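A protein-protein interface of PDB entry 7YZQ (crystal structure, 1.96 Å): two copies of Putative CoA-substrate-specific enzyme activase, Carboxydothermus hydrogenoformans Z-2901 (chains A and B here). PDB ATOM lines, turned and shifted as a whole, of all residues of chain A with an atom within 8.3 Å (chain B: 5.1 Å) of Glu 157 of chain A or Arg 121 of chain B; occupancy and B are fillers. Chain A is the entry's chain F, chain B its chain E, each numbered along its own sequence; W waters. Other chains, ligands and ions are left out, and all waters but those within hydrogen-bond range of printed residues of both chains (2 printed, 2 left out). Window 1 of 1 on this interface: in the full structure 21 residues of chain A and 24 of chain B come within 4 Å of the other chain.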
ATOM      1  N   ARG A 121      -5.424 -11.188  12.039  1.00  0.00           N
ATOM      2  CA  ARG A 121      -6.555 -10.879  12.906  1.00  0.00           C
ATOM      3  C   ARG A 121      -6.195  -9.818  13.942  1.00  0.00           C
ATOM      4  O   ARG A 121      -7.016  -8.956  14.269  1.00  0.00           O
ATOM      5  CB  ARG A 121      -7.050 -12.166  13.559  1.00  0.00           C
ATOM      6  CG  ARG A 121      -7.958 -11.985  14.744  1.00  0.00           C
ATOM      7  CD  ARG A 121      -9.314 -11.372  14.351  1.00  0.00           C
ATOM      8  NE  ARG A 121     -10.268 -11.537  15.456  1.00  0.00           N
ATOM      9  CZ  ARG A 121     -11.410 -10.859  15.601  1.00  0.00           C
ATOM     10  NH1 ARG A 121     -12.187 -11.108  16.658  1.00  0.00           N
ATOM     11  NH2 ARG A 121     -11.786  -9.943  14.697  1.00  0.00           N
ATOM     12  N   PHE A 122      -4.976  -9.841  14.465  1.00  0.00           N
ATOM     13  CA  PHE A 122      -4.613  -8.838  15.455  1.00  0.00           C
ATOM     14  C   PHE A 122      -4.624  -7.448  14.848  1.00  0.00           C
ATOM     15  O   PHE A 122      -5.087  -6.490  15.485  1.00  0.00           O
ATOM     16  CB  PHE A 122      -3.228  -9.151  16.027  1.00  0.00           C
ATOM     17  CG  PHE A 122      -2.680  -8.099  16.948  1.00  0.00           C
ATOM     18  CD1 PHE A 122      -3.303  -7.831  18.116  1.00  0.00           C
ATOM     19  CD2 PHE A 122      -1.502  -7.430  16.652  1.00  0.00           C
ATOM     20  CE1 PHE A 122      -2.773  -6.874  19.000  1.00  0.00           C
ATOM     21  CE2 PHE A 122      -0.978  -6.485  17.494  1.00  0.00           C
ATOM     22  CZ  PHE A 122      -1.608  -6.222  18.691  1.00  0.00           C
ATOM     23  N   GLU A 124      -6.421  -6.351  12.352  1.00  0.00           N
ATOM     24  CA  GLU A 124      -7.819  -5.947  12.228  1.00  0.00           C
ATOM     25  C   GLU A 124      -8.375  -5.500  13.587  1.00  0.00           C
ATOM     26  O   GLU A 124      -8.964  -4.420  13.718  1.00  0.00           O
ATOM     27  CB  GLU A 124      -8.629  -7.115  11.646  1.00  0.00           C
ATOM     28  CG  GLU A 124     -10.064  -6.753  11.287  1.00  0.00           C
ATOM     29  CD  GLU A 124     -10.956  -7.972  10.939  1.00  0.00           C
ATOM     30  OE1 GLU A 124     -10.422  -9.062  10.609  1.00  0.00           O
ATOM     31  OE2 GLU A 124     -12.204  -7.816  10.982  1.00  0.00           O
ATOM     32  N   ILE A 125      -8.205  -6.331  14.618  1.00  0.00           N
ATOM     33  CA  ILE A 125      -8.678  -5.976  15.958  1.00  0.00           C
ATOM     34  C   ILE A 125      -8.133  -4.618  16.364  1.00  0.00           C
ATOM     35  O   ILE A 125      -8.880  -3.733  16.792  1.00  0.00           O
ATOM     36  CB  ILE A 125      -8.265  -7.060  16.972  1.00  0.00           C
ATOM     37  CG1 ILE A 125      -9.127  -8.296  16.785  1.00  0.00           C
ATOM     38  CG2 ILE A 125      -8.300  -6.523  18.389  1.00  0.00           C
ATOM     39  CD1 ILE A 125      -8.500  -9.559  17.356  1.00  0.00           C
ATOM     40  N   ILE A 126      -6.818  -4.438  16.232  1.00  0.00           N
ATOM     41  CA  ILE A 126      -6.158  -3.226  16.721  1.00  0.00           C
ATOM     42  C   ILE A 126      -6.613  -1.998  15.938  1.00  0.00           C
ATOM     43  O   ILE A 126      -6.901  -0.937  16.517  1.00  0.00           O
ATOM     44  CB  ILE A 126      -4.631  -3.387  16.644  1.00  0.00           C
ATOM     45  CG1 ILE A 126      -4.153  -4.179  17.853  1.00  0.00           C
ATOM     46  CG2 ILE A 126      -3.976  -2.035  16.583  1.00  0.00           C
ATOM     47  CD1 ILE A 126      -4.236  -3.437  19.178  1.00  0.00           C
ATOM     48  N   THR A 128      -9.375  -1.551  14.425  1.00  0.00           N
ATOM     49  CA  THR A 128     -10.720  -1.266  14.912  1.00  0.00           C
ATOM     50  C   THR A 128     -10.657  -0.524  16.237  1.00  0.00           C
ATOM     51  O   THR A 128     -11.232   0.560  16.382  1.00  0.00           O
ATOM     52  CB  THR A 128     -11.525  -2.555  15.084  1.00  0.00           C
ATOM     53  OG1 THR A 128     -11.691  -3.212  13.819  1.00  0.00           O
ATOM     54  CG2 THR A 128     -12.887  -2.260  15.664  1.00  0.00           C
ATOM     55  N   ALA A 129      -9.961  -1.110  17.218  1.00  0.00           N
ATOM     56  CA  ALA A 129      -9.927  -0.536  18.560  1.00  0.00           C
ATOM     57  C   ALA A 129      -9.407   0.889  18.527  1.00  0.00           C
ATOM     58  O   ALA A 129     -10.026   1.806  19.069  1.00  0.00           O
ATOM     59  CB  ALA A 129      -9.056  -1.388  19.478  1.00  0.00           C
ATOM     60  N   ILE A 130      -8.239   1.086  17.910  1.00  0.00           N
ATOM     61  CA  ILE A 130      -7.695   2.430  17.769  1.00  0.00           C
ATOM     62  C   ILE A 130      -8.385   3.173  16.641  1.00  0.00           C
ATOM     63  O   ILE A 130      -7.971   4.287  16.285  1.00  0.00           O
ATOM     64  CB  ILE A 130      -6.183   2.430  17.477  1.00  0.00           C
ATOM     65  CG1 ILE A 130      -5.458   1.321  18.221  1.00  0.00           C
ATOM     66  CG2 ILE A 130      -5.595   3.719  17.865  1.00  0.00           C
ATOM     67  CD1 ILE A 130      -3.987   1.168  17.795  1.00  0.00           C
ATOM     68  N   ILE A 148       7.451  -1.964  17.777  1.00  0.00           N
ATOM     69  CA  ILE A 148       6.617  -2.789  18.630  1.00  0.00           C
ATOM     70  C   ILE A 148       7.176  -4.194  18.578  1.00  0.00           C
ATOM     71  O   ILE A 148       7.742  -4.621  17.570  1.00  0.00           O
ATOM     72  CB  ILE A 148       5.125  -2.699  18.223  1.00  0.00           C
ATOM     73  CG1 ILE A 148       4.675  -1.239  18.520  1.00  0.00           C
ATOM     74  CG2 ILE A 148       4.297  -3.713  18.964  1.00  0.00           C
ATOM     75  CD1 ILE A 148       3.220  -1.008  18.573  1.00  0.00           C
ATOM     76  N   ASN A 149       7.072  -4.894  19.700  1.00  0.00           N
ATOM     77  CA  ASN A 149       7.666  -6.224  19.802  1.00  0.00           C
ATOM     78  C   ASN A 149       7.157  -7.110  18.678  1.00  0.00           C
ATOM     79  O   ASN A 149       5.968  -7.106  18.353  1.00  0.00           O
ATOM     80  CB  ASN A 149       7.333  -6.848  21.167  1.00  0.00           C
ATOM     81  CG  ASN A 149       8.309  -7.916  21.581  1.00  0.00           C
ATOM     82  OD1 ASN A 149       8.749  -8.715  20.765  1.00  0.00           O
ATOM     83  ND2 ASN A 149       8.654  -7.938  22.871  1.00  0.00           N
ATOM     84  N   CYS A 152       5.165 -11.840  19.142  1.00  0.00           N
ATOM     85  CA  CYS A 152       3.837 -12.416  18.997  1.00  0.00           C
ATOM     86  C   CYS A 152       2.852 -11.305  19.280  1.00  0.00           C
ATOM     87  O   CYS A 152       3.224 -10.217  19.738  1.00  0.00           O
ATOM     88  CB  CYS A 152       3.647 -13.591  19.955  1.00  0.00           C
ATOM     89  SG  CYS A 152       3.733 -13.006  21.680  1.00  0.00           S
ATOM     90  N   THR A 153       1.583 -11.609  19.041  1.00  0.00           N
ATOM     91  CA  THR A 153       0.541 -10.613  19.229  1.00  0.00           C
ATOM     92  C   THR A 153       0.207 -10.380  20.707  1.00  0.00           C
ATOM     93  O   THR A 153      -0.332  -9.318  21.030  1.00  0.00           O
ATOM     94  CB  THR A 153      -0.761 -10.984  18.486  1.00  0.00           C
ATOM     95  OG1 THR A 153      -1.280 -12.184  19.030  1.00  0.00           O
ATOM     96  CG2 THR A 153      -0.530 -11.145  17.017  1.00  0.00           C
ATOM     97  N   VAL A 154       0.530 -11.327  21.601  1.00  0.00           N
ATOM     98  CA  VAL A 154       0.348 -11.096  23.029  1.00  0.00           C
ATOM     99  C   VAL A 154       1.280  -9.994  23.507  1.00  0.00           C
ATOM    100  O   VAL A 154       0.848  -9.049  24.172  1.00  0.00           O
ATOM    101  CB  VAL A 154       0.594 -12.391  23.813  1.00  0.00           C
ATOM    102  CG1 VAL A 154       0.595 -12.115  25.304  1.00  0.00           C
ATOM    103  CG2 VAL A 154      -0.484 -13.411  23.503  1.00  0.00           C
ATOM    104  N   PHE A 155       2.587 -10.130  23.203  1.00  0.00           N
ATOM    105  CA  PHE A 155       3.560  -9.118  23.621  1.00  0.00           C
ATOM    106  C   PHE A 155       3.299  -7.781  22.920  1.00  0.00           C
ATOM    107  O   PHE A 155       3.566  -6.713  23.480  1.00  0.00           O
ATOM    108  CB  PHE A 155       4.989  -9.576  23.307  1.00  0.00           C
ATOM    109  CG  PHE A 155       5.502 -10.734  24.130  1.00  0.00           C
ATOM    110  CD1 PHE A 155       4.659 -11.596  24.756  1.00  0.00           C
ATOM    111  CD2 PHE A 155       6.876 -10.939  24.250  1.00  0.00           C
ATOM    112  CE1 PHE A 155       5.144 -12.683  25.502  1.00  0.00           C
ATOM    113  CE2 PHE A 155       7.388 -11.988  24.970  1.00  0.00           C
ATOM    114  CZ  PHE A 155       6.512 -12.885  25.608  1.00  0.00           C
ATOM    115  N   ALA A 156       2.816  -7.827  21.674  1.00  0.00           N
ATOM    116  CA  ALA A 156       2.541  -6.598  20.951  1.00  0.00           C
ATOM    117  C   ALA A 156       1.352  -5.863  21.568  1.00  0.00           C
ATOM    118  O   ALA A 156       1.391  -4.645  21.712  1.00  0.00           O
ATOM    119  CB  ALA A 156       2.295  -6.889  19.467  1.00  0.00           C
ATOM    120  N   GLU A 157       0.294  -6.587  21.932  1.00  0.00           N
ATOM    121  CA  GLU A 157      -0.851  -5.976  22.610  1.00  0.00           C
ATOM    122  C   GLU A 157      -0.414  -5.318  23.916  1.00  0.00           C
ATOM    123  O   GLU A 157      -0.789  -4.179  24.209  1.00  0.00           O
ATOM    124  CB  GLU A 157      -1.929  -7.031  22.870  1.00  0.00           C
ATOM    125  CG  GLU A 157      -3.189  -6.445  23.469  1.00  0.00           C
ATOM    126  CD  GLU A 157      -4.226  -7.505  23.839  1.00  0.00           C
ATOM    127  OE1 GLU A 157      -5.422  -7.157  23.899  1.00  0.00           O
ATOM    128  OE2 GLU A 157      -3.852  -8.679  24.083  1.00  0.00           O
ATOM    129  N   SER A 158       0.379  -6.021  24.725  1.00  0.00           N
ATOM    130  CA  SER A 158       0.859  -5.427  25.970  1.00  0.00           C
ATOM    131  C   SER A 158       1.541  -4.089  25.713  1.00  0.00           C
ATOM    132  O   SER A 158       1.428  -3.162  26.515  1.00  0.00           O
ATOM    133  CB  SER A 158       1.825  -6.384  26.669  1.00  0.00           C
ATOM    134  OG  SER A 158       1.194  -7.621  26.939  1.00  0.00           O
ATOM    135  N   GLU A 159       2.323  -3.989  24.639  1.00  0.00           N
ATOM    136  CA  GLU A 159       3.049  -2.744  24.383  1.00  0.00           C
ATOM    137  C   GLU A 159       2.115  -1.670  23.867  1.00  0.00           C
ATOM    138  O   GLU A 159       2.242  -0.492  24.227  1.00  0.00           O
ATOM    139  CB  GLU A 159       4.189  -2.964  23.382  1.00  0.00           C
ATOM    140  CG  GLU A 159       5.356  -3.682  23.962  1.00  0.00           C
ATOM    141  CD  GLU A 159       6.515  -3.783  23.018  1.00  0.00           C
ATOM    142  OE1 GLU A 159       6.347  -3.521  21.805  1.00  0.00           O
ATOM    143  OE2 GLU A 159       7.609  -4.078  23.509  1.00  0.00           O
ATOM    144  N   VAL A 160       1.156  -2.062  23.029  1.00  0.00           N
ATOM    145  CA  VAL A 160       0.139  -1.122  22.565  1.00  0.00           C
ATOM    146  C   VAL A 160      -0.581  -0.486  23.745  1.00  0.00           C
ATOM    147  O   VAL A 160      -0.790   0.737  23.780  1.00  0.00           O
ATOM    148  CB  VAL A 160      -0.852  -1.830  21.616  1.00  0.00           C
ATOM    149  CG1 VAL A 160      -2.087  -0.940  21.350  1.00  0.00           C
ATOM    150  CG2 VAL A 160      -0.132  -2.179  20.324  1.00  0.00           C
ATOM    151  N   ILE A 161      -0.947  -1.294  24.747  1.00  0.00           N
ATOM    152  CA  ILE A 161      -1.613  -0.749  25.930  1.00  0.00           C
ATOM    153  C   ILE A 161      -0.695   0.219  26.662  1.00  0.00           C
ATOM    154  O   ILE A 161      -1.107   1.317  27.035  1.00  0.00           O
ATOM    155  CB  ILE A 161      -2.085  -1.888  26.859  1.00  0.00           C
ATOM    156  CG1 ILE A 161      -3.252  -2.660  26.222  1.00  0.00           C
ATOM    157  CG2 ILE A 161      -2.430  -1.352  28.221  1.00  0.00           C
ATOM    158  CD1 ILE A 161      -3.509  -4.013  26.887  1.00  0.00           C
ATOM    159  N   SER A 162       0.575  -0.157  26.848  1.00  0.00           N
ATOM    160  CA  SER A 162       1.525   0.723  27.532  1.00  0.00           C
ATOM    161  C   SER A 162       1.741   2.038  26.787  1.00  0.00           C
ATOM    162  O   SER A 162       1.869   3.108  27.415  1.00  0.00           O
ATOM    163  CB  SER A 162       2.890   0.022  27.712  1.00  0.00           C
ATOM    164  OG  SER A 162       2.828  -0.938  28.722  1.00  0.00           O
ATOM    165  N   LEU A 163       1.847   1.978  25.454  1.00  0.00           N
ATOM    166  CA  LEU A 163       2.154   3.188  24.696  1.00  0.00           C
ATOM    167  C   LEU A 163       0.979   4.162  24.733  1.00  0.00           C
ATOM    168  O   LEU A 163       1.148   5.364  24.919  1.00  0.00           O
ATOM    169  CB  LEU A 163       2.503   2.836  23.246  1.00  0.00           C
ATOM    170  CG  LEU A 163       3.900   2.203  23.056  1.00  0.00           C
ATOM    171  CD1 LEU A 163       3.971   1.449  21.761  1.00  0.00           C
ATOM    172  CD2 LEU A 163       4.951   3.274  23.132  1.00  0.00           C
ATOM    173  N   LEU A 164      -0.213   3.670  24.494  1.00  0.00           N
ATOM    174  CA  LEU A 164      -1.380   4.544  24.525  1.00  0.00           C
ATOM    175  C   LEU A 164      -1.645   5.032  25.938  1.00  0.00           C
ATOM    176  O   LEU A 164      -1.917   6.219  26.131  1.00  0.00           O
ATOM    177  CB  LEU A 164      -2.583   3.817  23.951  1.00  0.00           C
ATOM    178  CG  LEU A 164      -2.361   3.503  22.457  1.00  0.00           C
ATOM    179  CD1 LEU A 164      -3.453   2.671  21.827  1.00  0.00           C
ATOM    180  CD2 LEU A 164      -2.183   4.805  21.664  1.00  0.00           C
ATOM    181  N   VAL A 173       1.624   4.645  16.956  1.00  0.00           N
ATOM    182  CA  VAL A 173       1.495   3.239  17.313  1.00  0.00           C
ATOM    183  C   VAL A 173       1.112   2.422  16.089  1.00  0.00           C
ATOM    184  O   VAL A 173       1.638   1.330  15.860  1.00  0.00           O
ATOM    185  CB  VAL A 173       0.463   3.067  18.447  1.00  0.00           C
ATOM    186  CG1 VAL A 173      -0.025   1.613  18.521  1.00  0.00           C
ATOM    187  CG2 VAL A 173       1.056   3.503  19.791  1.00  0.00           C
ATOM    188  N   LEU A 177       3.159  -0.568  14.314  1.00  0.00           N
ATOM    189  CA  LEU A 177       2.709  -1.947  14.147  1.00  0.00           C
ATOM    190  C   LEU A 177       2.909  -2.443  12.715  1.00  0.00           C
ATOM    191  O   LEU A 177       3.358  -3.569  12.501  1.00  0.00           O
ATOM    192  CB  LEU A 177       1.242  -2.073  14.536  1.00  0.00           C
ATOM    193  CG  LEU A 177       0.966  -2.126  16.037  1.00  0.00           C
ATOM    194  CD1 LEU A 177      -0.512  -2.313  16.225  1.00  0.00           C
ATOM    195  CD2 LEU A 177       1.753  -3.253  16.722  1.00  0.00           C
ATOM    196  N   TYR B  32      -8.657   3.099  24.943  1.00  0.00           N
ATOM    197  CA  TYR B  32      -7.240   3.350  24.766  1.00  0.00           C
ATOM    198  C   TYR B  32      -6.859   4.808  24.975  1.00  0.00           C
ATOM    199  O   TYR B  32      -5.815   5.226  24.504  1.00  0.00           O
ATOM    200  CB  TYR B  32      -6.791   2.885  23.375  1.00  0.00           C
ATOM    201  CG  TYR B  32      -6.733   1.409  23.250  1.00  0.00           C
ATOM    202  CD1 TYR B  32      -5.600   0.721  23.665  1.00  0.00           C
ATOM    203  CD2 TYR B  32      -7.819   0.680  22.762  1.00  0.00           C
ATOM    204  CE1 TYR B  32      -5.522  -0.686  23.562  1.00  0.00           C
ATOM    205  CE2 TYR B  32      -7.758  -0.695  22.660  1.00  0.00           C
ATOM    206  CZ  TYR B  32      -6.591  -1.380  23.049  1.00  0.00           C
ATOM    207  OH  TYR B  32      -6.503  -2.758  22.951  1.00  0.00           O
ATOM    208  N   GLY B  91      -8.498  -8.655  35.049  1.00  0.00           N
ATOM    209  CA  GLY B  91      -8.803  -7.531  34.223  1.00  0.00           C
ATOM    210  C   GLY B  91      -8.653  -7.890  32.766  1.00  0.00           C
ATOM    211  O   GLY B  91      -8.592  -9.067  32.402  1.00  0.00           O
ATOM    212  N   GLY B  92      -8.602  -6.861  31.917  1.00  0.00           N
ATOM    213  CA  GLY B  92      -8.519  -7.116  30.491  1.00  0.00           C
ATOM    214  C   GLY B  92      -7.134  -7.543  30.019  1.00  0.00           C
ATOM    215  O   GLY B  92      -7.000  -8.321  29.065  1.00  0.00           O
ATOM    216  N   GLN B  93      -6.089  -7.098  30.698  1.00  0.00           N
ATOM    217  CA  GLN B  93      -4.726  -7.433  30.311  1.00  0.00           C
ATOM    218  C   GLN B  93      -3.912  -8.137  31.395  1.00  0.00           C
ATOM    219  O   GLN B  93      -2.949  -8.844  31.052  1.00  0.00           O
ATOM    220  CB  GLN B  93      -4.023  -6.143  29.853  1.00  0.00           C
ATOM    221  CG  GLN B  93      -2.511  -6.135  29.910  1.00  0.00           C
ATOM    222  CD  GLN B  93      -1.845  -6.809  28.740  1.00  0.00           C
ATOM    223  OE1 GLN B  93      -2.464  -7.205  27.708  1.00  0.00           O
ATOM    224  NE2 GLN B  93      -0.554  -6.991  28.902  1.00  0.00           N
ATOM    225  N   GLY B 118      -3.371 -10.609  28.712  1.00  0.00           N
ATOM    226  CA  GLY B 118      -4.462 -10.436  27.786  1.00  0.00           C
ATOM    227  C   GLY B 118      -5.579 -11.457  27.903  1.00  0.00           C
ATOM    228  O   GLY B 118      -6.441 -11.513  27.009  1.00  0.00           O
ATOM    229  N   THR B 119      -5.627 -12.223  28.998  1.00  0.00           N
ATOM    230  CA  THR B 119      -6.657 -13.256  29.142  1.00  0.00           C
ATOM    231  C   THR B 119      -8.061 -12.664  29.076  1.00  0.00           C
ATOM    232  O   THR B 119      -8.934 -13.170  28.363  1.00  0.00           O
ATOM    233  CB  THR B 119      -6.483 -14.004  30.458  1.00  0.00           C
ATOM    234  OG1 THR B 119      -5.195 -14.596  30.503  1.00  0.00           O
ATOM    235  CG2 THR B 119      -7.557 -15.084  30.602  1.00  0.00           C
ATOM    236  N   GLY B 120      -8.304 -11.605  29.831  1.00  0.00           N
ATOM    237  CA  GLY B 120      -9.642 -11.055  29.904  1.00  0.00           C
ATOM    238  C   GLY B 120     -10.114 -10.494  28.580  1.00  0.00           C
ATOM    239  O   GLY B 120     -11.253 -10.726  28.166  1.00  0.00           O
ATOM    240  N   ARG B 121      -9.223  -9.791  27.872  1.00  0.00           N
ATOM    241  CA  ARG B 121      -9.593  -9.181  26.596  1.00  0.00           C
ATOM    242  C   ARG B 121      -9.858 -10.251  25.552  1.00  0.00           C
ATOM    243  O   ARG B 121     -10.733 -10.095  24.695  1.00  0.00           O
ATOM    244  CB  ARG B 121      -8.489  -8.228  26.150  1.00  0.00           C
ATOM    245  CG  ARG B 121      -8.552  -7.804  24.730  1.00  0.00           C
ATOM    246  CD  ARG B 121      -9.458  -6.610  24.541  1.00  0.00           C
ATOM    247  NE  ARG B 121      -9.537  -6.231  23.121  1.00  0.00           N
ATOM    248  CZ  ARG B 121     -10.635  -5.791  22.494  1.00  0.00           C
ATOM    249  NH1 ARG B 121     -11.785  -5.631  23.147  1.00  0.00           N
ATOM    250  NH2 ARG B 121     -10.575  -5.501  21.194  1.00  0.00           N
ATOM    251  N   PHE B 122      -9.117 -11.351  25.620  1.00  0.00           N
ATOM    252  CA  PHE B 122      -9.355 -12.463  24.708  1.00  0.00           C
ATOM    253  C   PHE B 122     -10.716 -13.099  25.001  1.00  0.00           C
ATOM    254  O   PHE B 122     -11.474 -13.416  24.073  1.00  0.00           O
ATOM    255  CB  PHE B 122      -8.190 -13.468  24.818  1.00  0.00           C
ATOM    256  CG  PHE B 122      -8.457 -14.780  24.179  1.00  0.00           C
ATOM    257  CD1 PHE B 122      -8.481 -14.898  22.804  1.00  0.00           C
ATOM    258  CD2 PHE B 122      -8.677 -15.890  24.946  1.00  0.00           C
ATOM    259  CE1 PHE B 122      -8.753 -16.108  22.212  1.00  0.00           C
ATOM    260  CE2 PHE B 122      -8.961 -17.125  24.354  1.00  0.00           C
ATOM    261  CZ  PHE B 122      -9.005 -17.230  23.000  1.00  0.00           C
ATOM    262  N   LEU B 123     -11.054 -13.280  26.287  1.00  0.00           N
ATOM    263  CA  LEU B 123     -12.385 -13.788  26.632  1.00  0.00           C
ATOM    264  C   LEU B 123     -13.456 -12.855  26.090  1.00  0.00           C
ATOM    265  O   LEU B 123     -14.435 -13.301  25.477  1.00  0.00           O
ATOM    266  CB  LEU B 123     -12.559 -13.945  28.148  1.00  0.00           C
ATOM    267  CG  LEU B 123     -11.781 -15.090  28.797  1.00  0.00           C
ATOM    268  CD1 LEU B 123     -11.808 -14.997  30.279  1.00  0.00           C
ATOM    269  CD2 LEU B 123     -12.310 -16.433  28.326  1.00  0.00           C
ATOM    270  N   GLU B 124     -13.288 -11.547  26.307  1.00  0.00           N
ATOM    271  CA  GLU B 124     -14.252 -10.570  25.789  1.00  0.00           C
ATOM    272  C   GLU B 124     -14.412 -10.708  24.269  1.00  0.00           C
ATOM    273  O   GLU B 124     -15.530 -10.714  23.737  1.00  0.00           O
ATOM    274  CB  GLU B 124     -13.799  -9.153  26.172  1.00  0.00           C
ATOM    275  CG  GLU B 124     -14.774  -8.060  25.830  1.00  0.00           C
ATOM    276  CD  GLU B 124     -14.182  -6.638  26.033  1.00  0.00           C
ATOM    277  OE1 GLU B 124     -12.928  -6.486  26.049  1.00  0.00           O
ATOM    278  OE2 GLU B 124     -14.973  -5.666  26.171  1.00  0.00           O
ATOM    279  N   ILE B 125     -13.298 -10.820  23.552  1.00  0.00           N
ATOM    280  CA  ILE B 125     -13.330 -10.819  22.094  1.00  0.00           C
ATOM    281  C   ILE B 125     -13.983 -12.091  21.573  1.00  0.00           C
ATOM    282  O   ILE B 125     -14.898 -12.052  20.745  1.00  0.00           O
ATOM    283  CB  ILE B 125     -11.907 -10.655  21.529  1.00  0.00           C
ATOM    284  CG1 ILE B 125     -11.482  -9.191  21.565  1.00  0.00           C
ATOM    285  CG2 ILE B 125     -11.872 -11.167  20.132  1.00  0.00           C
ATOM    286  CD1 ILE B 125     -10.006  -9.011  21.262  1.00  0.00           C
ATOM    287  N   ILE B 126     -13.529 -13.241  22.054  1.00  0.00           N
ATOM    288  CA  ILE B 126     -13.987 -14.481  21.440  1.00  0.00           C
ATOM    289  C   ILE B 126     -15.443 -14.737  21.785  1.00  0.00           C
ATOM    290  O   ILE B 126     -16.185 -15.319  20.983  1.00  0.00           O
ATOM    291  CB  ILE B 126     -13.051 -15.644  21.847  1.00  0.00           C
ATOM    292  CG1 ILE B 126     -12.968 -16.690  20.719  1.00  0.00           C
ATOM    293  CG2 ILE B 126     -13.512 -16.321  23.100  1.00  0.00           C
ATOM    294  CD1 ILE B 126     -11.946 -16.403  19.664  1.00  0.00           C
HETATM  295  O   HOH W   1      -5.770 -10.493  24.485  1.00  0.00           O
HETATM  296  O   HOH W   2      -4.098   7.376  24.925  1.00  0.00           O
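The side-chain amide nitrogen (NE2) of Gln 93 of chain B sits at hydrogen-bond distance from the side-chain hydroxyl (OG) of Ser 158 of chain A, at 2.7 Å.
The side-chain carboxylate of Glu 124 of chain B is in salt-bridge range of the guanidinium group of Arg 121 of chain B, 3.2 Å away. O of Gln 93 of chain B is in hydrogen-bond range of N of Gly 118 of chain B (3.0 Å). N of Arg 121 of chain B sits at hydrogen-bond distance from O of Gly 92 of chain B (2.9 Å). The backbone carbonyl oxygen (O) of Ser 158 of chain A sits at hydrogen-bond distance from the side-chain hydroxyl (OG) of Ser 162 of chain A (3.4 Å). The backbone carbonyl oxygen (O) of Val 154 of chain A sits at hydrogen-bond distance from the side-chain hydroxyl (OG) of Ser 158 of chain A, 3.1 Å away.
Glu 157 of chain A touches just one residue of chain B: Arg 121. Of chain A, only Ile 125 and Glu 157 come within 4 Å of Arg 121 of chain B. No residue of chain A comes within 4 Å of Gly 120 of chain B. Printed residues of chain B within 4 Å of Arg 121 of chain A: Ile 125. Of the printed residues of chain B, Ile 125 of chain A touches Arg 121 (3.8 Å). Ile 148 of chain A touches none of the printed residues of chain B. Ile 130 of chain A touches none of the printed residues of chain B. The nearest printed residue of chain B that does not touch Glu 157 of chain A is Gly 118 of chain B (4.1 Å). The nearest printed residue of chain A that does not touch Tyr 32 of chain B is Ile 161 of chain A (4.02 Å).
Arg 121 of chain A touches Ile 125 of chain B, and with the chains exchanged Ile 125 of chain A touches Arg 121 of chain B. Positions printed for both chains: 121, 122, 124, 125 and 126. Of the 7 pairs that touch across the chains among the printed residues, 2 have their exchanged pair printed and touching as well.
Water W1 bridges OE2 of Glu 157 of chain A (2.7 Å) and O of Gly 118 of chain B (2.8 Å). Water W2 lies within hydrogen-bond range of O of Leu 164 of chain A and O of Tyr 32 of chain B.
Printed residues of chain A that touch a printed residue of chain B: Arg 121, Ile 125, Ala 129, Glu 157, Ser 158, Ile 161 and Leu 164. Hydrophobic or aromatic side chains of chain A that line the printed part of chain B: Ile 125, Ala 129, Ile 161 and Leu 164. Along chain A the printed residues that touch a printed residue of chain B span positions 121 to 164. Printed residues of chain B that touch a printed residue of chain A: Tyr 32, Gln 93, Arg 121 and Ile 125. Hydrophobic or aromatic side chains of chain B that line the printed part of chain A: Tyr 32 and Ile 125. Among the printed residues, no Asp or Glu carboxylate lies within 4 Å of a Lys or Arg side-chain nitrogen of the other chain.
Among the printed residues, merely in contact across the chains: Glu 157 of chain A with Arg 121 of chain B, Leu 164 of chain A with Tyr 32 of chain B, Ile 161 of chain A with Gln 93 of chain B, Arg 121 of chain A with Ile 125 of chain B, Ala 129 of chain A with Tyr 32 of chain B and Ile 125 of chain A with Arg 121 of chain B.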
